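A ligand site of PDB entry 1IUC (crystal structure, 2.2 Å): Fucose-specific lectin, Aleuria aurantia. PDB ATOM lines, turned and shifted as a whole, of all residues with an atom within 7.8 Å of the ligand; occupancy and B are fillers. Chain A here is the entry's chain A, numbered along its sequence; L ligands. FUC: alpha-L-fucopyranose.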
ATOM      1  N   ILE A 173      15.888 -24.745  21.757  1.00  0.00           N
ATOM      2  CA  ILE A 173      16.331 -24.189  20.468  1.00  0.00           C
ATOM      3  C   ILE A 173      15.427 -24.615  19.316  1.00  0.00           C
ATOM      4  O   ILE A 173      15.488 -24.052  18.220  1.00  0.00           O
ATOM      5  CB  ILE A 173      17.785 -24.582  20.152  1.00  0.00           C
ATOM      6  CG1 ILE A 173      17.877 -26.094  19.906  1.00  0.00           C
ATOM      7  CG2 ILE A 173      18.693 -24.168  21.308  1.00  0.00           C
ATOM      8  CD1 ILE A 173      19.242 -26.530  19.419  1.00  0.00           C
ATOM      9  N   ARG A 177      14.170 -29.884  21.123  1.00  0.00           N
ATOM     10  CA  ARG A 177      15.639 -29.773  21.110  1.00  0.00           C
ATOM     11  C   ARG A 177      16.036 -28.850  22.262  1.00  0.00           C
ATOM     12  O   ARG A 177      15.777 -27.633  22.239  1.00  0.00           O
ATOM     13  CB  ARG A 177      16.138 -29.200  19.782  1.00  0.00           C
ATOM     14  CG  ARG A 177      15.787 -30.046  18.571  1.00  0.00           C
ATOM     15  CD  ARG A 177      16.455 -29.480  17.323  1.00  0.00           C
ATOM     16  NE  ARG A 177      17.912 -29.659  17.367  1.00  0.00           N
ATOM     17  CZ  ARG A 177      18.769 -28.995  16.594  1.00  0.00           C
ATOM     18  NH1 ARG A 177      18.322 -28.115  15.711  1.00  0.00           N
ATOM     19  NH2 ARG A 177      20.073 -29.221  16.699  1.00  0.00           N
ATOM     20  N   LEU A 178      16.684 -29.429  23.260  1.00  0.00           N
ATOM     21  CA  LEU A 178      17.057 -28.698  24.464  1.00  0.00           C
ATOM     22  C   LEU A 178      18.550 -28.516  24.659  1.00  0.00           C
ATOM     23  O   LEU A 178      19.354 -29.387  24.305  1.00  0.00           O
ATOM     24  CB  LEU A 178      16.483 -29.445  25.686  1.00  0.00           C
ATOM     25  CG  LEU A 178      15.119 -30.113  25.450  1.00  0.00           C
ATOM     26  CD1 LEU A 178      14.675 -30.841  26.712  1.00  0.00           C
ATOM     27  CD2 LEU A 178      14.094 -29.053  25.053  1.00  0.00           C
ATOM     28  N   ARG A 179      18.924 -27.381  25.232  1.00  0.00           N
ATOM     29  CA  ARG A 179      20.313 -27.049  25.533  1.00  0.00           C
ATOM     30  C   ARG A 179      20.337 -26.505  26.960  1.00  0.00           C
ATOM     31  O   ARG A 179      19.611 -25.572  27.291  1.00  0.00           O
ATOM     32  CB  ARG A 179      20.834 -25.991  24.558  1.00  0.00           C
ATOM     33  CG  ARG A 179      20.943 -26.495  23.117  1.00  0.00           C
ATOM     34  CD  ARG A 179      22.000 -27.594  23.004  1.00  0.00           C
ATOM     35  NE  ARG A 179      22.139 -28.105  21.639  1.00  0.00           N
ATOM     36  CZ  ARG A 179      21.305 -28.967  21.064  1.00  0.00           C
ATOM     37  NH1 ARG A 179      20.254 -29.429  21.723  1.00  0.00           N
ATOM     38  NH2 ARG A 179      21.526 -29.363  19.818  1.00  0.00           N
ATOM     39  N   ILE A 180      21.181 -27.087  27.804  1.00  0.00           N
ATOM     40  CA  ILE A 180      21.297 -26.660  29.205  1.00  0.00           C
ATOM     41  C   ILE A 180      22.740 -26.249  29.443  1.00  0.00           C
ATOM     42  O   ILE A 180      23.662 -26.956  29.031  1.00  0.00           O
ATOM     43  CB  ILE A 180      20.989 -27.821  30.173  1.00  0.00           C
ATOM     44  CG1 ILE A 180      19.691 -28.518  29.765  1.00  0.00           C
ATOM     45  CG2 ILE A 180      20.928 -27.292  31.608  1.00  0.00           C
ATOM     46  CD1 ILE A 180      18.460 -27.674  29.923  1.00  0.00           C
ATOM     47  N   TYR A 181      22.937 -25.106  30.099  1.00  0.00           N
ATOM     48  CA  TYR A 181      24.282 -24.624  30.398  1.00  0.00           C
ATOM     49  C   TYR A 181      24.486 -24.499  31.889  1.00  0.00           C
ATOM     50  O   TYR A 181      23.624 -23.984  32.608  1.00  0.00           O
ATOM     51  CB  TYR A 181      24.546 -23.282  29.707  1.00  0.00           C
ATOM     52  CG  TYR A 181      24.310 -23.354  28.218  1.00  0.00           C
ATOM     53  CD1 TYR A 181      23.027 -23.189  27.686  1.00  0.00           C
ATOM     54  CD2 TYR A 181      25.356 -23.667  27.343  1.00  0.00           C
ATOM     55  CE1 TYR A 181      22.785 -23.335  26.332  1.00  0.00           C
ATOM     56  CE2 TYR A 181      25.118 -23.817  25.973  1.00  0.00           C
ATOM     57  CZ  TYR A 181      23.837 -23.658  25.485  1.00  0.00           C
ATOM     58  OH  TYR A 181      23.605 -23.810  24.148  1.00  0.00           O
ATOM     59  N   GLU A 191      27.785 -27.577  28.289  1.00  0.00           N
ATOM     60  CA  GLU A 191      26.501 -27.661  27.627  1.00  0.00           C
ATOM     61  C   GLU A 191      26.009 -29.107  27.521  1.00  0.00           C
ATOM     62  O   GLU A 191      26.783 -29.998  27.165  1.00  0.00           O
ATOM     63  CB  GLU A 191      26.629 -27.050  26.240  1.00  0.00           C
ATOM     64  CG  GLU A 191      25.455 -27.258  25.319  1.00  0.00           C
ATOM     65  CD  GLU A 191      25.795 -26.865  23.895  1.00  0.00           C
ATOM     66  OE1 GLU A 191      26.798 -27.402  23.377  1.00  0.00           O
ATOM     67  OE2 GLU A 191      25.069 -26.043  23.291  1.00  0.00           O
ATOM     68  N   HIS A 192      24.737 -29.328  27.827  1.00  0.00           N
ATOM     69  CA  HIS A 192      24.185 -30.674  27.710  1.00  0.00           C
ATOM     70  C   HIS A 192      23.074 -30.573  26.684  1.00  0.00           C
ATOM     71  O   HIS A 192      22.326 -29.604  26.675  1.00  0.00           O
ATOM     72  CB  HIS A 192      23.625 -31.173  29.041  1.00  0.00           C
ATOM     73  CG  HIS A 192      24.016 -32.576  29.331  1.00  0.00           C
ATOM     74  ND1 HIS A 192      25.294 -32.939  29.707  1.00  0.00           N
ATOM     75  CD2 HIS A 192      23.316 -33.734  29.250  1.00  0.00           C
ATOM     76  CE1 HIS A 192      25.371 -34.249  29.827  1.00  0.00           C
ATOM     77  NE2 HIS A 192      24.185 -34.762  29.557  1.00  0.00           N
ATOM     78  N   CYS A 193      22.977 -31.578  25.813  1.00  0.00           N
ATOM     79  CA  CYS A 193      21.978 -31.522  24.740  1.00  0.00           C
ATOM     80  C   CYS A 193      21.004 -32.685  24.636  1.00  0.00           C
ATOM     81  O   CYS A 193      21.318 -33.818  25.001  1.00  0.00           O
ATOM     82  CB  CYS A 193      22.686 -31.397  23.388  1.00  0.00           C
ATOM     83  SG  CYS A 193      24.164 -30.345  23.381  1.00  0.00           S
ATOM     84  N   ASP A 195      18.433 -33.743  21.474  1.00  0.00           N
ATOM     85  CA  ASP A 195      17.923 -33.403  20.157  1.00  0.00           C
ATOM     86  C   ASP A 195      16.691 -34.203  19.768  1.00  0.00           C
ATOM     87  O   ASP A 195      15.826 -33.714  19.024  1.00  0.00           O
ATOM     88  CB  ASP A 195      19.022 -33.573  19.108  1.00  0.00           C
ATOM     89  CG  ASP A 195      19.891 -32.339  18.971  1.00  0.00           C
ATOM     90  OD1 ASP A 195      21.042 -32.466  18.508  1.00  0.00           O
ATOM     91  OD2 ASP A 195      19.416 -31.239  19.325  1.00  0.00           O
ATOM     92  N   TYR A 200      23.362 -35.768  25.631  1.00  0.00           N
ATOM     93  CA  TYR A 200      24.772 -35.897  25.294  1.00  0.00           C
ATOM     94  C   TYR A 200      25.486 -34.569  25.516  1.00  0.00           C
ATOM     95  O   TYR A 200      24.896 -33.499  25.390  1.00  0.00           O
ATOM     96  CB  TYR A 200      24.925 -36.373  23.837  1.00  0.00           C
ATOM     97  CG  TYR A 200      24.477 -35.381  22.777  1.00  0.00           C
ATOM     98  CD1 TYR A 200      25.341 -34.394  22.305  1.00  0.00           C
ATOM     99  CD2 TYR A 200      23.183 -35.430  22.244  1.00  0.00           C
ATOM    100  CE1 TYR A 200      24.943 -33.478  21.333  1.00  0.00           C
ATOM    101  CE2 TYR A 200      22.777 -34.516  21.277  1.00  0.00           C
ATOM    102  CZ  TYR A 200      23.655 -33.538  20.829  1.00  0.00           C
ATOM    103  OH  TYR A 200      23.250 -32.614  19.890  1.00  0.00           O
ATOM    104  N   VAL A 201      26.773 -34.654  25.868  1.00  0.00           N
ATOM    105  CA  VAL A 201      27.580 -33.468  26.104  1.00  0.00           C
ATOM    106  C   VAL A 201      27.721 -32.661  24.820  1.00  0.00           C
ATOM    107  O   VAL A 201      28.101 -33.198  23.780  1.00  0.00           O
ATOM    108  CB  VAL A 201      28.989 -33.868  26.608  1.00  0.00           C
ATOM    109  CG1 VAL A 201      29.823 -32.629  26.872  1.00  0.00           C
ATOM    110  CG2 VAL A 201      28.871 -34.684  27.887  1.00  0.00           C
ATOM    111  N   GLY A 202      27.419 -31.367  24.901  1.00  0.00           N
ATOM    112  CA  GLY A 202      27.512 -30.497  23.730  1.00  0.00           C
ATOM    113  C   GLY A 202      28.936 -30.048  23.480  1.00  0.00           C
ATOM    114  O   GLY A 202      29.811 -30.287  24.301  1.00  0.00           O
ATOM    115  N   GLY A 203      29.159 -29.388  22.361  1.00  0.00           N
ATOM    116  CA  GLY A 203      30.504 -28.930  22.027  1.00  0.00           C
ATOM    117  C   GLY A 203      30.929 -27.632  22.679  1.00  0.00           C
ATOM    118  O   GLY A 203      32.125 -27.363  22.778  1.00  0.00           O
ATOM    119  N   PHE A 204      29.969 -26.821  23.128  1.00  0.00           N
ATOM    120  CA  PHE A 204      30.301 -25.551  23.764  1.00  0.00           C
ATOM    121  C   PHE A 204      31.061 -25.699  25.067  1.00  0.00           C
ATOM    122  O   PHE A 204      30.784 -26.583  25.876  1.00  0.00           O
ATOM    123  CB  PHE A 204      29.057 -24.723  24.046  1.00  0.00           C
ATOM    124  CG  PHE A 204      29.359 -23.416  24.726  1.00  0.00           C
ATOM    125  CD1 PHE A 204      30.090 -22.432  24.063  1.00  0.00           C
ATOM    126  CD2 PHE A 204      28.952 -23.177  26.037  1.00  0.00           C
ATOM    127  CE1 PHE A 204      30.410 -21.233  24.691  1.00  0.00           C
ATOM    128  CE2 PHE A 204      29.255 -21.982  26.674  1.00  0.00           C
ATOM    129  CZ  PHE A 204      29.987 -21.007  26.007  1.00  0.00           C
ATOM    130  N   SER A 205      32.005 -24.791  25.275  1.00  0.00           N
ATOM    131  CA  SER A 205      32.828 -24.791  26.474  1.00  0.00           C
ATOM    132  C   SER A 205      33.489 -23.429  26.606  1.00  0.00           C
ATOM    133  O   SER A 205      33.901 -22.834  25.607  1.00  0.00           O
ATOM    134  CB  SER A 205      33.897 -25.873  26.347  1.00  0.00           C
ATOM    135  OG  SER A 205      34.770 -25.848  27.452  1.00  0.00           O
ATOM    136  N   THR A 222      18.486 -21.259  12.279  1.00  0.00           N
ATOM    137  CA  THR A 222      19.844 -21.776  12.279  1.00  0.00           C
ATOM    138  C   THR A 222      20.135 -22.924  13.238  1.00  0.00           C
ATOM    139  O   THR A 222      20.726 -23.939  12.834  1.00  0.00           O
ATOM    140  CB  THR A 222      20.854 -20.639  12.510  1.00  0.00           C
ATOM    141  OG1 THR A 222      20.606 -19.606  11.543  1.00  0.00           O
ATOM    142  CG2 THR A 222      22.272 -21.145  12.344  1.00  0.00           C
ATOM    143  N   PRO A 223      19.776 -22.794  14.529  1.00  0.00           N
ATOM    144  CA  PRO A 223      19.142 -21.661  15.210  1.00  0.00           C
ATOM    145  C   PRO A 223      20.253 -20.836  15.863  1.00  0.00           C
ATOM    146  O   PRO A 223      21.411 -21.253  15.874  1.00  0.00           O
ATOM    147  CB  PRO A 223      18.277 -22.352  16.247  1.00  0.00           C
ATOM    148  CG  PRO A 223      19.217 -23.438  16.735  1.00  0.00           C
ATOM    149  CD  PRO A 223      19.851 -23.968  15.436  1.00  0.00           C
ATOM    150  N   ASN A 224      19.899 -19.673  16.390  1.00  0.00           N
ATOM    151  CA  ASN A 224      20.879 -18.809  17.050  1.00  0.00           C
ATOM    152  C   ASN A 224      20.720 -18.976  18.562  1.00  0.00           C
ATOM    153  O   ASN A 224      19.604 -19.060  19.072  1.00  0.00           O
ATOM    154  CB  ASN A 224      20.627 -17.359  16.670  1.00  0.00           C
ATOM    155  CG  ASN A 224      20.594 -17.168  15.172  1.00  0.00           C
ATOM    156  OD1 ASN A 224      21.641 -17.070  14.513  1.00  0.00           O
ATOM    157  ND2 ASN A 224      19.390 -17.118  14.611  1.00  0.00           N
ATOM    158  N   ILE A 225      21.844 -19.024  19.257  1.00  0.00           N
ATOM    159  CA  ILE A 225      21.843 -19.185  20.702  1.00  0.00           C
ATOM    160  C   ILE A 225      22.776 -18.137  21.300  1.00  0.00           C
ATOM    161  O   ILE A 225      23.839 -17.857  20.724  1.00  0.00           O
ATOM    162  CB  ILE A 225      22.386 -20.569  21.117  1.00  0.00           C
ATOM    163  CG1 ILE A 225      21.643 -21.683  20.393  1.00  0.00           C
ATOM    164  CG2 ILE A 225      22.262 -20.746  22.628  1.00  0.00           C
ATOM    165  CD1 ILE A 225      22.351 -23.016  20.484  1.00  0.00           C
ATOM    166  N   TYR A 241      26.108 -18.279  19.288  1.00  0.00           N
ATOM    167  CA  TYR A 241      26.100 -19.378  18.329  1.00  0.00           C
ATOM    168  C   TYR A 241      25.217 -18.944  17.171  1.00  0.00           C
ATOM    169  O   TYR A 241      24.075 -18.514  17.376  1.00  0.00           O
ATOM    170  CB  TYR A 241      25.519 -20.640  18.969  1.00  0.00           C
ATOM    171  CG  TYR A 241      25.383 -21.810  18.022  1.00  0.00           C
ATOM    172  CD1 TYR A 241      26.395 -22.759  17.906  1.00  0.00           C
ATOM    173  CD2 TYR A 241      24.222 -21.981  17.254  1.00  0.00           C
ATOM    174  CE1 TYR A 241      26.269 -23.848  17.057  1.00  0.00           C
ATOM    175  CE2 TYR A 241      24.087 -23.063  16.388  1.00  0.00           C
ATOM    176  CZ  TYR A 241      25.113 -24.003  16.304  1.00  0.00           C
ATOM    177  OH  TYR A 241      24.983 -25.087  15.470  1.00  0.00           O
ATOM    178  N   GLY A 243      25.524 -20.918  14.128  1.00  0.00           N
ATOM    179  CA  GLY A 243      25.830 -22.004  13.230  1.00  0.00           C
ATOM    180  C   GLY A 243      27.078 -22.660  13.782  1.00  0.00           C
ATOM    181  O   GLY A 243      27.413 -23.817  13.488  1.00  0.00           O
ATOM    182  N   SER A 244      27.781 -21.900  14.616  1.00  0.00           N
ATOM    183  CA  SER A 244      29.007 -22.307  15.274  1.00  0.00           C
ATOM    184  C   SER A 244      29.241 -21.255  16.363  1.00  0.00           C
ATOM    185  O   SER A 244      28.684 -20.162  16.288  1.00  0.00           O
ATOM    186  CB  SER A 244      30.166 -22.314  14.277  1.00  0.00           C
ATOM    187  OG  SER A 244      30.227 -21.075  13.594  1.00  0.00           O
ATOM    188  N   TRP A 245      30.070 -21.572  17.353  1.00  0.00           N
ATOM    189  CA  TRP A 245      30.316 -20.627  18.444  1.00  0.00           C
ATOM    190  C   TRP A 245      31.448 -19.640  18.204  1.00  0.00           C
ATOM    191  O   TRP A 245      32.486 -20.008  17.667  1.00  0.00           O
ATOM    192  CB  TRP A 245      30.618 -21.390  19.738  1.00  0.00           C
ATOM    193  CG  TRP A 245      29.478 -22.215  20.252  1.00  0.00           C
ATOM    194  CD1 TRP A 245      29.281 -23.562  20.069  1.00  0.00           C
ATOM    195  CD2 TRP A 245      28.366 -21.752  21.039  1.00  0.00           C
ATOM    196  NE1 TRP A 245      28.125 -23.962  20.704  1.00  0.00           N
ATOM    197  CE2 TRP A 245      27.548 -22.871  21.300  1.00  0.00           C
ATOM    198  CE3 TRP A 245      27.995 -20.496  21.550  1.00  0.00           C
ATOM    199  CZ2 TRP A 245      26.359 -22.772  22.056  1.00  0.00           C
ATOM    200  CZ3 TRP A 245      26.825 -20.394  22.297  1.00  0.00           C
ATOM    201  CH2 TRP A 245      26.024 -21.537  22.538  1.00  0.00           C
HETATM  202  C1  FUC L   1      25.178 -29.297  19.003  1.00  0.00           C
HETATM  203  C2  FUC L   1      26.092 -28.668  20.103  1.00  0.00           C
HETATM  204  C3  FUC L   1      26.413 -27.191  19.759  1.00  0.00           C
HETATM  205  C4  FUC L   1      25.072 -26.399  19.571  1.00  0.00           C
HETATM  206  C5  FUC L   1      24.265 -27.060  18.420  1.00  0.00           C
HETATM  207  C6  FUC L   1      22.933 -26.379  18.136  1.00  0.00           C
HETATM  208  O1  FUC L   1      25.869 -29.431  17.820  1.00  0.00           O
HETATM  209  O2  FUC L   1      27.292 -29.407  20.284  1.00  0.00           O
HETATM  210  O3  FUC L   1      27.241 -26.628  20.775  1.00  0.00           O
HETATM  211  O4  FUC L   1      24.281 -26.481  20.757  1.00  0.00           O
HETATM  212  O5  FUC L   1      23.986 -28.463  18.742  1.00  0.00           O
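Merely in contact with the ligand: Ile 173 (3.9 Å), Tyr 200 (3.9 Å), Gly 202 (3.6 Å), Phe 204 (3.6 Å), Ile 225 (3.98 Å) and Tyr 241 (3.6 Å). Hydrophobic or aromatic side chains that line the ligand: Ile 173, Ile 225, Tyr 241 and Trp 245. Within 4 Å of the ligand: Ile 173, Arg 179, Glu 191, Tyr 200, Gly 202, Gly 203, Phe 204, Ile 225, Tyr 241 and Trp 245. The nearest printed residue that does not touch the ligand is Cys 193 (4.2 Å).
O of Tyr 200 lies within hydrogen-bond range of N of Cys 193 (2.7 Å). The backbone carbonyl oxygen of Glu 191 sits at hydrogen-bond distance from the backbone NH of Gly 202, at 2.7 Å. The side-chain hydroxyl (OH) of Tyr 200 is in hydrogen-bond range of the side-chain carboxylate (OD1) of Asp 195 (2.6 Å). The guanidinium group (NE) of Arg 179 is in salt-bridge range of the side-chain carboxylate (OE2) of Glu 191 (3.9 Å). OE2 of Glu 191 lies within hydrogen-bond range of OH of Tyr 181 (2.8 Å). NE of Arg 179 is in hydrogen-bond range of SG of Cys 193 (3.5 Å). OE1 of Glu 191 lies within hydrogen-bond range of N of Phe 204, 3.2 Å away. The backbone NH (N) of Gly 203 sits at hydrogen-bond distance from the side-chain carboxylate (OE1) of Glu 191 (3.2 Å).
NE of Arg 179 lies within hydrogen-bond range of O4 of the ligand. The side-chain carboxylate of Glu 191 is in hydrogen-bond range of an oxygen (O4) of the ligand, at 2.7 Å. O2 of the ligand sits at hydrogen-bond distance from N of Gly 203 (2.8 Å). NE1 of Trp 245 is in hydrogen-bond range of O3 of the ligand (2.8 Å).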
